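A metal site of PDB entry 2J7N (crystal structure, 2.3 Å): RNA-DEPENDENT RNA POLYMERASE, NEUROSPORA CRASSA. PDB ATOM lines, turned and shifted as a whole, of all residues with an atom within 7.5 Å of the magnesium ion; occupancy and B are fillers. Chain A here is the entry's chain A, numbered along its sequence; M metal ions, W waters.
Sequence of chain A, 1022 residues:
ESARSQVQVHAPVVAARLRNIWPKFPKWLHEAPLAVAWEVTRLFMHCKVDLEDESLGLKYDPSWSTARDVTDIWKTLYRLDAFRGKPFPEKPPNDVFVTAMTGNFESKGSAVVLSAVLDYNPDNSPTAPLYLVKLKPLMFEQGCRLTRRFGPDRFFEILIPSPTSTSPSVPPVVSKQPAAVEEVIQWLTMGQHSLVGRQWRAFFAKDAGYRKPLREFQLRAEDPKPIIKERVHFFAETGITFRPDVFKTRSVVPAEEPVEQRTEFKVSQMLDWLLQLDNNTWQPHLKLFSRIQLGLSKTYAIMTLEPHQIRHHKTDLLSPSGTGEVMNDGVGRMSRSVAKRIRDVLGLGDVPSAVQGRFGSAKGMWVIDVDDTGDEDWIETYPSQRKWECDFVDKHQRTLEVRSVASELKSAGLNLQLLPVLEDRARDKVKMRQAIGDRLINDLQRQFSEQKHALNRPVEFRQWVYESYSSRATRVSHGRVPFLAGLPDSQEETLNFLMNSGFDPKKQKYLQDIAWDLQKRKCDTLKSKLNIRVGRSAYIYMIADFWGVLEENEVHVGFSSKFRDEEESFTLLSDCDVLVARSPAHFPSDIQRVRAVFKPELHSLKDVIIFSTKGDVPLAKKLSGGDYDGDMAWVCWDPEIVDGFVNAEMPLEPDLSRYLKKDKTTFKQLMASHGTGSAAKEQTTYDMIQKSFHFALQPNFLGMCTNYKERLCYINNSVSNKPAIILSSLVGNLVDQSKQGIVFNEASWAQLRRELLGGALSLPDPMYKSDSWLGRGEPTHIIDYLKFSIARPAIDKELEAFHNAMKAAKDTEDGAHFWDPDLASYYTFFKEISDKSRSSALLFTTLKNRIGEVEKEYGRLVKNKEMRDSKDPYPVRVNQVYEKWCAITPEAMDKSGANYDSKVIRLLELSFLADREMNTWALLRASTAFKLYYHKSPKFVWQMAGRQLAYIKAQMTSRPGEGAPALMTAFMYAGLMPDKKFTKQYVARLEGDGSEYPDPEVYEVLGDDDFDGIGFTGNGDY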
ATOM      1  N   ASP A 329     -12.847  21.555  -4.796  1.00  0.00           N
ATOM      2  CA  ASP A 329     -12.146  21.296  -3.564  1.00  0.00           C
ATOM      3  C   ASP A 329     -11.734  22.578  -2.828  1.00  0.00           C
ATOM      4  O   ASP A 329     -10.779  23.237  -3.227  1.00  0.00           O
ATOM      5  CB  ASP A 329     -10.929  20.428  -3.863  1.00  0.00           C
ATOM      6  CG  ASP A 329     -10.285  19.820  -2.640  1.00  0.00           C
ATOM      7  OD1 ASP A 329     -10.409  20.349  -1.493  1.00  0.00           O
ATOM      8  OD2 ASP A 329      -9.578  18.815  -2.842  1.00  0.00           O
ATOM      9  N   GLY A 330     -12.450  22.907  -1.756  1.00  0.00           N
ATOM     10  CA  GLY A 330     -12.071  24.030  -0.894  1.00  0.00           C
ATOM     11  C   GLY A 330     -12.811  25.322  -1.168  1.00  0.00           C
ATOM     12  O   GLY A 330     -12.538  26.375  -0.525  1.00  0.00           O
ATOM     13  N   GLN A 356     -10.692  34.593   0.956  1.00  0.00           N
ATOM     14  CA  GLN A 356     -10.127  33.430   1.656  1.00  0.00           C
ATOM     15  C   GLN A 356     -10.541  33.524   3.099  1.00  0.00           C
ATOM     16  O   GLN A 356     -10.396  34.563   3.715  1.00  0.00           O
ATOM     17  CB  GLN A 356      -8.603  33.335   1.575  1.00  0.00           C
ATOM     18  CG  GLN A 356      -8.076  31.949   1.952  1.00  0.00           C
ATOM     19  CD  GLN A 356      -6.543  31.879   2.055  1.00  0.00           C
ATOM     20  OE1 GLN A 356      -5.831  32.869   1.814  1.00  0.00           O
ATOM     21  NE2 GLN A 356      -6.024  30.716   2.426  1.00  0.00           N
ATOM     22  N   LYS A 363     -12.910  25.839   5.806  1.00  0.00           N
ATOM     23  CA  LYS A 363     -11.786  26.645   5.462  1.00  0.00           C
ATOM     24  C   LYS A 363     -11.678  26.642   3.930  1.00  0.00           C
ATOM     25  O   LYS A 363     -11.805  25.590   3.294  1.00  0.00           O
ATOM     26  CB  LYS A 363     -10.559  25.983   6.051  1.00  0.00           C
ATOM     27  CG  LYS A 363      -9.443  26.919   6.263  1.00  0.00           C
ATOM     28  CD  LYS A 363      -8.325  26.588   5.318  1.00  0.00           C
ATOM     29  CE  LYS A 363      -7.563  25.369   5.775  1.00  0.00           C
ATOM     30  NZ  LYS A 363      -6.399  25.241   4.875  1.00  0.00           N
ATOM     31  N   ARG A 582       0.812  26.832 -10.866  1.00  0.00           N
ATOM     32  CA  ARG A 582       1.016  27.199  -9.462  1.00  0.00           C
ATOM     33  C   ARG A 582       2.491  27.076  -9.173  1.00  0.00           C
ATOM     34  O   ARG A 582       3.140  26.119  -9.613  1.00  0.00           O
ATOM     35  CB  ARG A 582       0.270  26.250  -8.546  1.00  0.00           C
ATOM     36  CG  ARG A 582      -1.228  26.508  -8.420  1.00  0.00           C
ATOM     37  CD  ARG A 582      -1.669  26.096  -7.016  1.00  0.00           C
ATOM     38  NE  ARG A 582      -1.285  24.738  -6.668  1.00  0.00           N
ATOM     39  CZ  ARG A 582      -0.695  24.347  -5.541  1.00  0.00           C
ATOM     40  NH1 ARG A 582      -0.371  25.204  -4.578  1.00  0.00           N
ATOM     41  NH2 ARG A 582      -0.410  23.074  -5.377  1.00  0.00           N
ATOM     42  N   GLY A 625      -0.914  19.483  -8.004  1.00  0.00           N
ATOM     43  CA  GLY A 625      -1.872  19.018  -6.979  1.00  0.00           C
ATOM     44  C   GLY A 625      -2.554  20.122  -6.172  1.00  0.00           C
ATOM     45  O   GLY A 625      -2.800  19.969  -4.971  1.00  0.00           O
ATOM     46  N   GLY A 626      -2.876  21.254  -6.823  1.00  0.00           N
ATOM     47  CA  GLY A 626      -3.568  22.356  -6.148  1.00  0.00           C
ATOM     48  C   GLY A 626      -5.066  22.185  -5.975  1.00  0.00           C
ATOM     49  O   GLY A 626      -5.630  21.111  -6.259  1.00  0.00           O
ATOM     50  N   ASP A 627      -5.720  23.252  -5.501  1.00  0.00           N
ATOM     51  CA  ASP A 627      -7.167  23.281  -5.237  1.00  0.00           C
ATOM     52  C   ASP A 627      -7.676  24.704  -5.057  1.00  0.00           C
ATOM     53  O   ASP A 627      -6.961  25.666  -5.386  1.00  0.00           O
ATOM     54  CB  ASP A 627      -7.534  22.445  -4.005  1.00  0.00           C
ATOM     55  CG  ASP A 627      -6.818  22.913  -2.732  1.00  0.00           C
ATOM     56  OD1 ASP A 627      -6.086  23.939  -2.712  1.00  0.00           O
ATOM     57  OD2 ASP A 627      -7.013  22.211  -1.722  1.00  0.00           O
ATOM     58  N   TYR A 628      -8.868  24.852  -4.493  1.00  0.00           N
ATOM     59  CA  TYR A 628      -9.529  26.163  -4.463  1.00  0.00           C
ATOM     60  C   TYR A 628      -9.720  26.698  -3.080  1.00  0.00           C
ATOM     61  O   TYR A 628     -10.758  27.328  -2.774  1.00  0.00           O
ATOM     62  CB  TYR A 628     -10.878  26.111  -5.203  1.00  0.00           C
ATOM     63  CG  TYR A 628     -10.763  25.529  -6.600  1.00  0.00           C
ATOM     64  CD1 TYR A 628     -11.098  24.220  -6.833  1.00  0.00           C
ATOM     65  CD2 TYR A 628     -10.274  26.273  -7.664  1.00  0.00           C
ATOM     66  CE1 TYR A 628     -10.973  23.676  -8.087  1.00  0.00           C
ATOM     67  CE2 TYR A 628     -10.137  25.726  -8.925  1.00  0.00           C
ATOM     68  CZ  TYR A 628     -10.494  24.428  -9.129  1.00  0.00           C
ATOM     69  OH  TYR A 628     -10.387  23.830 -10.387  1.00  0.00           O
ATOM     70  N   ASP A 629      -8.727  26.473  -2.225  1.00  0.00           N
ATOM     71  CA  ASP A 629      -8.817  26.923  -0.850  1.00  0.00           C
ATOM     72  C   ASP A 629      -7.934  28.139  -0.584  1.00  0.00           C
ATOM     73  O   ASP A 629      -7.659  28.469   0.563  1.00  0.00           O
ATOM     74  CB  ASP A 629      -8.496  25.784   0.129  1.00  0.00           C
ATOM     75  CG  ASP A 629      -7.013  25.517   0.245  1.00  0.00           C
ATOM     76  OD1 ASP A 629      -6.197  26.069  -0.560  1.00  0.00           O
ATOM     77  OD2 ASP A 629      -6.653  24.739   1.150  1.00  0.00           O
ATOM     78  N   GLY A 630      -7.514  28.818  -1.643  1.00  0.00           N
ATOM     79  CA  GLY A 630      -6.650  29.961  -1.479  1.00  0.00           C
ATOM     80  C   GLY A 630      -5.478  29.929  -2.423  1.00  0.00           C
ATOM     81  O   GLY A 630      -4.718  30.890  -2.528  1.00  0.00           O
ATOM     82  N   ASP A 631      -5.339  28.820  -3.147  1.00  0.00           N
ATOM     83  CA  ASP A 631      -4.331  28.760  -4.206  1.00  0.00           C
ATOM     84  C   ASP A 631      -4.508  29.913  -5.198  1.00  0.00           C
ATOM     85  O   ASP A 631      -5.645  30.273  -5.521  1.00  0.00           O
ATOM     86  CB  ASP A 631      -4.410  27.463  -4.975  1.00  0.00           C
ATOM     87  CG  ASP A 631      -4.257  26.260  -4.113  1.00  0.00           C
ATOM     88  OD1 ASP A 631      -4.496  26.368  -2.887  1.00  0.00           O
ATOM     89  OD2 ASP A 631      -3.960  25.193  -4.673  1.00  0.00           O
ATOM     90  N   MET A 632      -3.385  30.463  -5.665  1.00  0.00           N
ATOM     91  CA  MET A 632      -3.354  31.427  -6.736  1.00  0.00           C
ATOM     92  C   MET A 632      -2.598  30.831  -7.918  1.00  0.00           C
ATOM     93  O   MET A 632      -1.585  30.126  -7.746  1.00  0.00           O
ATOM     94  CB  MET A 632      -2.667  32.707  -6.282  1.00  0.00           C
ATOM     95  CG  MET A 632      -3.353  33.338  -5.103  1.00  0.00           C
ATOM     96  SD  MET A 632      -2.583  34.874  -4.638  1.00  0.00           S
ATOM     97  CE  MET A 632      -3.539  36.148  -5.446  1.00  0.00           C
HETATM   98 MG    MG M   1      -4.750  24.790  -1.393  1.00  0.00          MG
HETATM   99  O   HOH W   1      -3.430  23.706  -2.499  1.00  0.00           O
HETATM  100  O   HOH W   2      -3.362  25.804  -0.121  1.00  0.00           O
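The side-chain amino group (NZ) of Lys 363 lies within salt-bridge range of the side-chain carboxylate (OD2) of Asp 629 (3.8 Å).
NE of Arg 582 is in salt-bridge range of OD2 of Asp 631 (3.4 Å).
NE2 of Gln 356 lies within hydrogen-bond range of O of Asp 629 (3.3 Å).
Water W1 binds the magnesium ion.
OD1 of Asp 627 binds the magnesium ion (2.1 Å).
OD1 of Asp 629 is bound to the magnesium ion.
The magnesium ion is bound by water W2 (2.1 Å).
The magnesium ion is bound by the side-chain carboxylate (OD1) of Asp 631, 2.2 Å away.
Three residues have an atom within 4 Å of the magnesium ion: Asp 627, Asp 629 and Asp 631.
The nearest printed residue that does not touch the magnesium ion is Gly 630 (4.9 Å).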
